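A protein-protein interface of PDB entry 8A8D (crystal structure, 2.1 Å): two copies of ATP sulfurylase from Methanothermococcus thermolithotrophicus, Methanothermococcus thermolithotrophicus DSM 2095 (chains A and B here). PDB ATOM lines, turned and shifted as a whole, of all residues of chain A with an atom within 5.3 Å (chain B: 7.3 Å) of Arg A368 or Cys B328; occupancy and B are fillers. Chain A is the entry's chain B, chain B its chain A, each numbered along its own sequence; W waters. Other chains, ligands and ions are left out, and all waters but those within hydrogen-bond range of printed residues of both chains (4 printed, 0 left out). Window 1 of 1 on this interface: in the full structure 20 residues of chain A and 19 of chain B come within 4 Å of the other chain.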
ATOM      1  N   LEU A 200      -2.911  27.530  27.953  1.00  0.00           N
ATOM      2  CA  LEU A 200      -1.672  26.793  27.730  1.00  0.00           C
ATOM      3  C   LEU A 200      -0.796  26.727  28.973  1.00  0.00           C
ATOM      4  O   LEU A 200       0.020  25.805  29.091  1.00  0.00           O
ATOM      5  CB  LEU A 200      -0.891  27.408  26.571  1.00  0.00           C
ATOM      6  CG  LEU A 200      -1.129  26.665  25.255  1.00  0.00           C
ATOM      7  CD1 LEU A 200      -2.489  27.045  24.689  1.00  0.00           C
ATOM      8  CD2 LEU A 200      -0.025  26.941  24.252  1.00  0.00           C
ATOM      9  N   GLU A 203      -2.029  23.583  30.850  1.00  0.00           N
ATOM     10  CA  GLU A 203      -1.518  22.397  30.170  1.00  0.00           C
ATOM     11  C   GLU A 203      -0.029  22.211  30.436  1.00  0.00           C
ATOM     12  O   GLU A 203       0.433  21.088  30.666  1.00  0.00           O
ATOM     13  CB  GLU A 203      -1.784  22.508  28.669  1.00  0.00           C
ATOM     14  CG  GLU A 203      -1.402  21.278  27.861  1.00  0.00           C
ATOM     15  CD  GLU A 203      -1.663  21.469  26.380  1.00  0.00           C
ATOM     16  OE1 GLU A 203      -2.356  22.446  26.027  1.00  0.00           O
ATOM     17  OE2 GLU A 203      -1.171  20.654  25.572  1.00  0.00           O
ATOM     18  N   LYS A 207       1.381  18.729  32.195  1.00  0.00           N
ATOM     19  CA  LYS A 207       2.294  17.854  31.469  1.00  0.00           C
ATOM     20  C   LYS A 207       3.674  17.827  32.110  1.00  0.00           C
ATOM     21  O   LYS A 207       4.356  16.797  32.064  1.00  0.00           O
ATOM     22  CB  LYS A 207       2.375  18.294  30.009  1.00  0.00           C
ATOM     23  CG  LYS A 207       1.161  17.861  29.203  1.00  0.00           C
ATOM     24  CD  LYS A 207       1.214  18.334  27.764  1.00  0.00           C
ATOM     25  CE  LYS A 207       0.014  17.811  26.990  1.00  0.00           C
ATOM     26  NZ  LYS A 207      -0.063  18.366  25.614  1.00  0.00           N
ATOM     27  N   LEU A 242      -9.589  19.388  25.093  1.00  0.00           N
ATOM     28  CA  LEU A 242      -8.142  19.463  25.269  1.00  0.00           C
ATOM     29  C   LEU A 242      -7.530  18.070  25.345  1.00  0.00           C
ATOM     30  O   LEU A 242      -6.580  17.755  24.620  1.00  0.00           O
ATOM     31  CB  LEU A 242      -7.813  20.266  26.528  1.00  0.00           C
ATOM     32  CG  LEU A 242      -6.339  20.328  26.929  1.00  0.00           C
ATOM     33  CD1 LEU A 242      -5.580  21.272  26.009  1.00  0.00           C
ATOM     34  CD2 LEU A 242      -6.197  20.756  28.381  1.00  0.00           C
ATOM     35  N   TYR A 246      -4.807  16.781  22.630  1.00  0.00           N
ATOM     36  CA  TYR A 246      -3.450  17.112  23.047  1.00  0.00           C
ATOM     37  C   TYR A 246      -2.869  16.219  24.133  1.00  0.00           C
ATOM     38  O   TYR A 246      -1.680  16.363  24.432  1.00  0.00           O
ATOM     39  CB  TYR A 246      -3.404  18.574  23.525  1.00  0.00           C
ATOM     40  CG  TYR A 246      -3.639  19.563  22.405  1.00  0.00           C
ATOM     41  CD1 TYR A 246      -4.923  19.955  22.051  1.00  0.00           C
ATOM     42  CD2 TYR A 246      -2.574  20.090  21.689  1.00  0.00           C
ATOM     43  CE1 TYR A 246      -5.139  20.850  21.020  1.00  0.00           C
ATOM     44  CE2 TYR A 246      -2.779  20.984  20.659  1.00  0.00           C
ATOM     45  CZ  TYR A 246      -4.063  21.361  20.328  1.00  0.00           C
ATOM     46  OH  TYR A 246      -4.265  22.253  19.301  1.00  0.00           O
ATOM     47  N   GLU A 364      -3.137  31.622  19.857  1.00  0.00           N
ATOM     48  CA  GLU A 364      -2.962  30.200  20.121  1.00  0.00           C
ATOM     49  C   GLU A 364      -1.846  29.925  21.119  1.00  0.00           C
ATOM     50  O   GLU A 364      -1.740  28.793  21.601  1.00  0.00           O
ATOM     51  CB  GLU A 364      -2.703  29.456  18.810  1.00  0.00           C
ATOM     52  CG  GLU A 364      -3.729  29.783  17.729  1.00  0.00           C
ATOM     53  CD  GLU A 364      -3.913  28.667  16.717  1.00  0.00           C
ATOM     54  OE1 GLU A 364      -3.303  27.591  16.883  1.00  0.00           O
ATOM     55  OE2 GLU A 364      -4.673  28.872  15.747  1.00  0.00           O
ATOM     56  N   PHE A 366      -2.031  31.362  23.915  1.00  0.00           N
ATOM     57  CA  PHE A 366      -2.832  31.429  25.132  1.00  0.00           C
ATOM     58  C   PHE A 366      -3.833  30.289  25.242  1.00  0.00           C
ATOM     59  O   PHE A 366      -4.087  29.804  26.343  1.00  0.00           O
ATOM     60  CB  PHE A 366      -3.606  32.754  25.203  1.00  0.00           C
ATOM     61  CG  PHE A 366      -2.848  33.899  25.844  1.00  0.00           C
ATOM     62  CD1 PHE A 366      -1.698  33.694  26.596  1.00  0.00           C
ATOM     63  CD2 PHE A 366      -3.312  35.197  25.691  1.00  0.00           C
ATOM     64  CE1 PHE A 366      -1.029  34.759  27.171  1.00  0.00           C
ATOM     65  CE2 PHE A 366      -2.647  36.264  26.263  1.00  0.00           C
ATOM     66  CZ  PHE A 366      -1.506  36.046  27.005  1.00  0.00           C
ATOM     67  N   MET A 367      -4.413  29.843  24.125  1.00  0.00           N
ATOM     68  CA  MET A 367      -5.522  28.897  24.169  1.00  0.00           C
ATOM     69  C   MET A 367      -5.536  28.062  22.898  1.00  0.00           C
ATOM     70  O   MET A 367      -5.440  28.604  21.795  1.00  0.00           O
ATOM     71  CB  MET A 367      -6.854  29.644  24.343  1.00  0.00           C
ATOM     72  CG  MET A 367      -8.091  28.878  23.895  1.00  0.00           C
ATOM     73  SD  MET A 367      -9.653  29.555  24.527  1.00  0.00           S
ATOM     74  CE  MET A 367      -9.268  29.868  26.251  1.00  0.00           C
ATOM     75  N   ARG A 368      -5.660  26.746  23.064  1.00  0.00           N
ATOM     76  CA  ARG A 368      -5.666  25.845  21.921  1.00  0.00           C
ATOM     77  C   ARG A 368      -6.811  26.189  20.978  1.00  0.00           C
ATOM     78  O   ARG A 368      -7.899  26.583  21.409  1.00  0.00           O
ATOM     79  CB  ARG A 368      -5.791  24.393  22.388  1.00  0.00           C
ATOM     80  CG  ARG A 368      -4.650  23.911  23.269  1.00  0.00           C
ATOM     81  CD  ARG A 368      -3.312  23.996  22.554  1.00  0.00           C
ATOM     82  NE  ARG A 368      -2.280  23.208  23.219  1.00  0.00           N
ATOM     83  CZ  ARG A 368      -1.022  23.127  22.809  1.00  0.00           C
ATOM     84  NH1 ARG A 368      -0.597  23.794  21.750  1.00  0.00           N
ATOM     85  NH2 ARG A 368      -0.171  22.353  23.476  1.00  0.00           N
ATOM     86  N   LYS A 369      -6.560  26.032  19.677  1.00  0.00           N
ATOM     87  CA  LYS A 369      -7.584  26.323  18.679  1.00  0.00           C
ATOM     88  C   LYS A 369      -8.860  25.539  18.958  1.00  0.00           C
ATOM     89  O   LYS A 369      -9.958  26.106  18.995  1.00  0.00           O
ATOM     90  CB  LYS A 369      -7.051  26.001  17.281  1.00  0.00           C
ATOM     91  CG  LYS A 369      -8.010  26.344  16.151  1.00  0.00           C
ATOM     92  CD  LYS A 369      -7.713  25.524  14.905  1.00  0.00           C
ATOM     93  CE  LYS A 369      -8.783  25.729  13.846  1.00  0.00           C
ATOM     94  NZ  LYS A 369      -9.410  24.445  13.419  1.00  0.00           N
ATOM     95  N   GLU A 370      -8.730  24.225  19.158  1.00  0.00           N
ATOM     96  CA  GLU A 370      -9.911  23.391  19.350  1.00  0.00           C
ATOM     97  C   GLU A 370     -10.632  23.725  20.650  1.00  0.00           C
ATOM     98  O   GLU A 370     -11.857  23.578  20.732  1.00  0.00           O
ATOM     99  CB  GLU A 370      -9.516  21.915  19.330  1.00  0.00           C
ATOM    100  CG  GLU A 370      -8.931  21.442  18.007  1.00  0.00           C
ATOM    101  CD  GLU A 370      -7.466  21.806  17.842  1.00  0.00           C
ATOM    102  OE1 GLU A 370      -6.902  22.443  18.758  1.00  0.00           O
ATOM    103  OE2 GLU A 370      -6.878  21.458  16.796  1.00  0.00           O
ATOM    104  N   VAL A 371      -9.898  24.169  21.671  1.00  0.00           N
ATOM    105  CA  VAL A 371     -10.533  24.556  22.925  1.00  0.00           C
ATOM    106  C   VAL A 371     -11.392  25.797  22.721  1.00  0.00           C
ATOM    107  O   VAL A 371     -12.541  25.862  23.176  1.00  0.00           O
ATOM    108  CB  VAL A 371      -9.473  24.779  24.019  1.00  0.00           C
ATOM    109  CG1 VAL A 371     -10.096  25.443  25.240  1.00  0.00           C
ATOM    110  CG2 VAL A 371      -8.821  23.461  24.397  1.00  0.00           C
ATOM    111  N   TYR A 372     -10.851  26.804  22.030  1.00  0.00           N
ATOM    112  CA  TYR A 372     -11.639  28.001  21.762  1.00  0.00           C
ATOM    113  C   TYR A 372     -12.884  27.666  20.953  1.00  0.00           C
ATOM    114  O   TYR A 372     -13.968  28.203  21.211  1.00  0.00           O
ATOM    115  CB  TYR A 372     -10.809  29.044  21.020  1.00  0.00           C
ATOM    116  CG  TYR A 372     -11.641  30.239  20.623  1.00  0.00           C
ATOM    117  CD1 TYR A 372     -12.013  31.186  21.566  1.00  0.00           C
ATOM    118  CD2 TYR A 372     -12.082  30.405  19.316  1.00  0.00           C
ATOM    119  CE1 TYR A 372     -12.784  32.275  21.220  1.00  0.00           C
ATOM    120  CE2 TYR A 372     -12.857  31.493  18.959  1.00  0.00           C
ATOM    121  CZ  TYR A 372     -13.206  32.424  19.917  1.00  0.00           C
ATOM    122  OH  TYR A 372     -13.977  33.512  19.578  1.00  0.00           O
ATOM    123  N   GLU A 373     -12.745  26.789  19.958  1.00  0.00           N
ATOM    124  CA  GLU A 373     -13.895  26.419  19.141  1.00  0.00           C
ATOM    125  C   GLU A 373     -14.961  25.727  19.979  1.00  0.00           C
ATOM    126  O   GLU A 373     -16.161  25.936  19.767  1.00  0.00           O
ATOM    127  CB  GLU A 373     -13.446  25.523  17.988  1.00  0.00           C
ATOM    128  CG  GLU A 373     -12.932  26.292  16.781  1.00  0.00           C
ATOM    129  CD  GLU A 373     -12.128  25.426  15.828  1.00  0.00           C
ATOM    130  OE1 GLU A 373     -11.852  24.254  16.166  1.00  0.00           O
ATOM    131  OE2 GLU A 373     -11.774  25.919  14.737  1.00  0.00           O
ATOM    132  N   TYR B 323      11.474  16.101  20.384  1.00  0.00           N
ATOM    133  CA  TYR B 323      11.226  16.487  19.005  1.00  0.00           C
ATOM    134  C   TYR B 323      10.284  17.678  19.002  1.00  0.00           C
ATOM    135  O   TYR B 323       9.608  17.959  19.995  1.00  0.00           O
ATOM    136  CB  TYR B 323      10.623  15.333  18.201  1.00  0.00           C
ATOM    137  CG  TYR B 323       9.380  14.752  18.836  1.00  0.00           C
ATOM    138  CD1 TYR B 323       8.126  15.288  18.575  1.00  0.00           C
ATOM    139  CD2 TYR B 323       9.462  13.672  19.705  1.00  0.00           C
ATOM    140  CE1 TYR B 323       6.989  14.762  19.156  1.00  0.00           C
ATOM    141  CE2 TYR B 323       8.330  13.139  20.292  1.00  0.00           C
ATOM    142  CZ  TYR B 323       7.096  13.688  20.013  1.00  0.00           C
ATOM    143  OH  TYR B 323       5.966  13.162  20.594  1.00  0.00           O
ATOM    144  N   TYR B 324      10.237  18.377  17.873  1.00  0.00           N
ATOM    145  CA  TYR B 324       9.269  19.446  17.694  1.00  0.00           C
ATOM    146  C   TYR B 324       7.977  18.864  17.137  1.00  0.00           C
ATOM    147  O   TYR B 324       8.001  18.087  16.176  1.00  0.00           O
ATOM    148  CB  TYR B 324       9.791  20.536  16.763  1.00  0.00           C
ATOM    149  CG  TYR B 324       8.869  21.732  16.727  1.00  0.00           C
ATOM    150  CD1 TYR B 324       8.996  22.755  17.655  1.00  0.00           C
ATOM    151  CD2 TYR B 324       7.853  21.823  15.787  1.00  0.00           C
ATOM    152  CE1 TYR B 324       8.153  23.843  17.637  1.00  0.00           C
ATOM    153  CE2 TYR B 324       7.001  22.909  15.761  1.00  0.00           C
ATOM    154  CZ  TYR B 324       7.156  23.915  16.690  1.00  0.00           C
ATOM    155  OH  TYR B 324       6.311  25.001  16.673  1.00  0.00           O
ATOM    156  N   CYS B 325       6.856  19.237  17.743  1.00  0.00           N
ATOM    157  CA  CYS B 325       5.537  18.827  17.282  1.00  0.00           C
ATOM    158  C   CYS B 325       4.833  20.021  16.657  1.00  0.00           C
ATOM    159  O   CYS B 325       4.724  21.081  17.284  1.00  0.00           O
ATOM    160  CB  CYS B 325       4.702  18.267  18.432  1.00  0.00           C
ATOM    161  SG  CYS B 325       3.051  17.763  17.933  1.00  0.00           S
ATOM    162  N   LYS B 326       4.352  19.846  15.428  1.00  0.00           N
ATOM    163  CA  LYS B 326       3.696  20.927  14.706  1.00  0.00           C
ATOM    164  C   LYS B 326       2.235  21.104  15.097  1.00  0.00           C
ATOM    165  O   LYS B 326       1.569  21.983  14.540  1.00  0.00           O
ATOM    166  CB  LYS B 326       3.812  20.691  13.199  1.00  0.00           C
ATOM    167  CG  LYS B 326       5.237  20.810  12.681  1.00  0.00           C
ATOM    168  CD  LYS B 326       5.326  20.520  11.193  1.00  0.00           C
ATOM    169  CE  LYS B 326       5.186  19.034  10.913  1.00  0.00           C
ATOM    170  NZ  LYS B 326       5.652  18.669   9.547  1.00  0.00           N
ATOM    171  N   LYS B 327       1.720  20.301  16.028  1.00  0.00           N
ATOM    172  CA  LYS B 327       0.405  20.546  16.609  1.00  0.00           C
ATOM    173  C   LYS B 327       0.506  21.114  18.020  1.00  0.00           C
ATOM    174  O   LYS B 327      -0.168  22.097  18.344  1.00  0.00           O
ATOM    175  CB  LYS B 327      -0.434  19.263  16.628  1.00  0.00           C
ATOM    176  CG  LYS B 327      -1.774  19.441  17.334  1.00  0.00           C
ATOM    177  CD  LYS B 327      -2.869  18.579  16.728  1.00  0.00           C
ATOM    178  CE  LYS B 327      -4.235  19.000  17.254  1.00  0.00           C
ATOM    179  NZ  LYS B 327      -5.298  18.006  16.948  1.00  0.00           N
ATOM    180  N   CYS B 328       1.342  20.514  18.871  1.00  0.00           N
ATOM    181  CA  CYS B 328       1.609  21.112  20.174  1.00  0.00           C
ATOM    182  C   CYS B 328       2.276  22.473  20.025  1.00  0.00           C
ATOM    183  O   CYS B 328       2.167  23.320  20.919  1.00  0.00           O
ATOM    184  CB  CYS B 328       2.490  20.189  21.015  1.00  0.00           C
ATOM    185  SG  CYS B 328       1.719  18.634  21.516  1.00  0.00           S
ATOM    186  N   ASN B 329       2.974  22.696  18.909  1.00  0.00           N
ATOM    187  CA  ASN B 329       3.694  23.944  18.658  1.00  0.00           C
ATOM    188  C   ASN B 329       4.831  24.142  19.657  1.00  0.00           C
ATOM    189  O   ASN B 329       5.110  25.262  20.090  1.00  0.00           O
ATOM    190  CB  ASN B 329       2.744  25.146  18.688  1.00  0.00           C
ATOM    191  CG  ASN B 329       1.675  25.076  17.617  1.00  0.00           C
ATOM    192  OD1 ASN B 329       1.935  24.644  16.493  1.00  0.00           O
ATOM    193  ND2 ASN B 329       0.464  25.498  17.960  1.00  0.00           N
ATOM    194  N   ALA B 330       5.504  23.052  20.021  1.00  0.00           N
ATOM    195  CA  ALA B 330       6.539  23.129  21.042  1.00  0.00           C
ATOM    196  C   ALA B 330       7.439  21.908  20.959  1.00  0.00           C
ATOM    197  O   ALA B 330       7.052  20.859  20.438  1.00  0.00           O
ATOM    198  CB  ALA B 330       5.930  23.235  22.446  1.00  0.00           C
ATOM    199  N   ILE B 331       8.656  22.064  21.479  1.00  0.00           N
ATOM    200  CA  ILE B 331       9.523  20.919  21.721  1.00  0.00           C
ATOM    201  C   ILE B 331       8.876  20.066  22.804  1.00  0.00           C
ATOM    202  O   ILE B 331       8.602  20.545  23.910  1.00  0.00           O
ATOM    203  CB  ILE B 331      10.932  21.370  22.126  1.00  0.00           C
ATOM    204  CG1 ILE B 331      11.569  22.172  20.988  1.00  0.00           C
ATOM    205  CG2 ILE B 331      11.796  20.169  22.490  1.00  0.00           C
ATOM    206  CD1 ILE B 331      13.006  22.564  21.241  1.00  0.00           C
ATOM    207  N   VAL B 332       8.623  18.799  22.490  1.00  0.00           N
ATOM    208  CA  VAL B 332       7.934  17.881  23.381  1.00  0.00           C
ATOM    209  C   VAL B 332       8.665  16.543  23.358  1.00  0.00           C
ATOM    210  O   VAL B 332       9.695  16.384  22.698  1.00  0.00           O
ATOM    211  CB  VAL B 332       6.453  17.695  22.991  1.00  0.00           C
ATOM    212  CG1 VAL B 332       5.704  19.011  23.098  1.00  0.00           C
ATOM    213  CG2 VAL B 332       6.344  17.133  21.578  1.00  0.00           C
ATOM    214  N   ILE B 336       4.351  13.131  26.635  1.00  0.00           N
ATOM    215  CA  ILE B 336       3.347  14.178  26.784  1.00  0.00           C
ATOM    216  C   ILE B 336       2.686  14.559  25.470  1.00  0.00           C
ATOM    217  O   ILE B 336       1.874  15.497  25.452  1.00  0.00           O
ATOM    218  CB  ILE B 336       3.949  15.431  27.451  1.00  0.00           C
ATOM    219  CG1 ILE B 336       5.100  15.988  26.609  1.00  0.00           C
ATOM    220  CG2 ILE B 336       4.437  15.102  28.855  1.00  0.00           C
ATOM    221  CD1 ILE B 336       5.597  17.340  27.078  1.00  0.00           C
ATOM    222  N   CYS B 337       2.999  13.874  24.373  1.00  0.00           N
ATOM    223  CA  CYS B 337       2.478  14.232  23.058  1.00  0.00           C
ATOM    224  C   CYS B 337       1.826  13.016  22.413  1.00  0.00           C
ATOM    225  O   CYS B 337       2.497  11.977  22.240  1.00  0.00           O
ATOM    226  CB  CYS B 337       3.595  14.775  22.165  1.00  0.00           C
ATOM    227  SG  CYS B 337       3.115  14.948  20.437  1.00  0.00           S
ATOM    228  N   PRO B 338       0.552  13.086  22.035  1.00  0.00           N
ATOM    229  CA  PRO B 338      -0.116  11.929  21.407  1.00  0.00           C
ATOM    230  C   PRO B 338      -0.134  11.930  19.883  1.00  0.00           C
ATOM    231  O   PRO B 338      -0.752  11.032  19.305  1.00  0.00           O
ATOM    232  CB  PRO B 338      -1.544  12.067  21.947  1.00  0.00           C
ATOM    233  CG  PRO B 338      -1.757  13.552  22.024  1.00  0.00           C
ATOM    234  CD  PRO B 338      -0.403  14.179  22.305  1.00  0.00           C
ATOM    235  N   HIS B 339       0.445  12.979  19.296  1.00  0.00           N
ATOM    236  CA  HIS B 339       0.410  13.269  17.837  1.00  0.00           C
ATOM    237  C   HIS B 339       1.198  12.262  16.993  1.00  0.00           C
ATOM    238  O   HIS B 339       2.231  11.763  17.457  1.00  0.00           O
ATOM    239  CB  HIS B 339       0.746  14.751  17.622  1.00  0.00           C
ATOM    240  CG  HIS B 339      -0.191  15.626  18.386  1.00  0.00           C
ATOM    241  ND1 HIS B 339       0.219  16.480  19.393  1.00  0.00           N
ATOM    242  CD2 HIS B 339      -1.535  15.730  18.327  1.00  0.00           C
ATOM    243  CE1 HIS B 339      -0.835  17.085  19.896  1.00  0.00           C
ATOM    244  NE2 HIS B 339      -1.917  16.647  19.258  1.00  0.00           N
ATOM    245  N   TYR B 343       3.223  15.205  12.277  1.00  0.00           N
ATOM    246  CA  TYR B 343       3.373  16.375  13.184  1.00  0.00           C
ATOM    247  C   TYR B 343       4.773  16.461  13.810  1.00  0.00           C
ATOM    248  O   TYR B 343       5.169  17.567  14.209  1.00  0.00           O
ATOM    249  CB  TYR B 343       2.261  16.384  14.237  1.00  0.00           C
ATOM    250  CG  TYR B 343       0.873  16.445  13.658  1.00  0.00           C
ATOM    251  CD1 TYR B 343       0.360  17.629  13.155  1.00  0.00           C
ATOM    252  CD2 TYR B 343       0.079  15.314  13.589  1.00  0.00           C
ATOM    253  CE1 TYR B 343      -0.912  17.692  12.611  1.00  0.00           C
ATOM    254  CE2 TYR B 343      -1.195  15.359  13.049  1.00  0.00           C
ATOM    255  CZ  TYR B 343      -1.693  16.551  12.559  1.00  0.00           C
ATOM    256  OH  TYR B 343      -2.945  16.596  12.024  1.00  0.00           O
HETATM  257  O   HOH W   1       0.965  27.633  20.197  1.00  0.00           O
HETATM  258  O   HOH W   2       2.523  18.290  24.570  1.00  0.00           O
HETATM  259  O   HOH W   3       2.915  22.858  23.912  1.00  0.00           O
HETATM  260  O   HOH W   4      -2.451  23.461  17.609  1.00  0.00           O
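No position is printed for both chains.
Of the 8 pairs that touch across the chains among the printed residues, none has its exchanged pair printed and touching as well.
O of Lys B327 touches CE2 of Tyr A246 (3.7 Å).
O of Ile B336 touches O of Tyr A246, 3.8 Å away.
Tyr A246 touches Pro B338 (O to CD, 3.3 Å).
Tyr A246 touches His B339.
NH1 of Arg A368 touches O of Lys B327, 3.8 Å away.
The backbone carbonyl oxygen of Ile B336 sits close to the side-chain amino group of Lys A207.
The side-chain amino group of Lys B327 is in salt-bridge range of the side-chain carboxylate of Glu A370 (3.8 Å).
The guanidinium group (NH1) of Arg A368 sits at hydrogen-bond distance from the backbone carbonyl oxygen (O) of Cys B328, 2.9 Å away.
The backbone carbonyl oxygen of Lys B327 sits at hydrogen-bond distance from the side-chain amide nitrogen of Asn B329 (3.5 Å).
The side-chain sulfur of Cys B325 sits close to the backbone NH of Lys B327.
The backbone carbonyl oxygen (O) of Tyr A246 sits at hydrogen-bond distance from the side-chain amino group (NZ) of Lys A207, 2.8 Å away.
The side-chain carboxylate of Glu A203 is in salt-bridge range of the guanidinium group of Arg A368 (2.9 Å).
OE2 of Glu A203 lies within salt-bridge range of NZ of Lys A207 (2.5 Å).
The side-chain carboxylate (OE1) of Glu A370 is in hydrogen-bond range of the side-chain hydroxyl (OH) of Tyr A246, 2.7 Å away.
Of the 15 printed residues of chain B, 5 touch a printed residue of chain A.
Hydrophobic or aromatic side chains of chain B within 4 Å of the printed part of chain A: Ile B336, Pro B338 and His B339.
Along chain B the printed residues that touch a printed residue of chain A span positions 327 to 339.
Of the 14 printed residues of chain A, 4 touch a printed residue of chain B.
Among the printed residues, Asp or Glu carboxylates within 4 Å of a Lys or Arg side-chain nitrogen of the other chain: Glu A370 with Lys B327.
Of the printed residues of chain B, Tyr A246 touches Lys B327, Ile B336, Pro B338 and His B339.
Arg A368 touches just these residues of chain B: Lys B327 and Cys B328.
Of the printed residues of chain A, His B339 touches Tyr A246.
The nearest residue of chain B that does not touch Arg A368 is Asn B329 (4.3 Å).
The nearest residue of chain A that does not touch Cys B328 is Tyr A246 (4.4 Å).
Water W4 bridges the side-chain hydroxyl of Tyr A246 (2.8 Å) and the backbone carbonyl oxygen of Lys B327 (2.8 Å).
Water W2 lies within hydrogen-bond range of the side-chain amino group of Lys A207 (2.8 Å) and the backbone carbonyl oxygen of Ile B336 (3.0 Å).
Water W3 lies within hydrogen-bond range of the backbone carbonyl oxygen of Cys B328 (3.1 Å) and the guanidinium group of Arg A368 (3.2 Å).
Water W1 lies within hydrogen-bond range of the side-chain amide nitrogen (ND2) of Asn B329 (3.1 Å) and the backbone carbonyl oxygen (O) of Glu A364 (3.3 Å).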
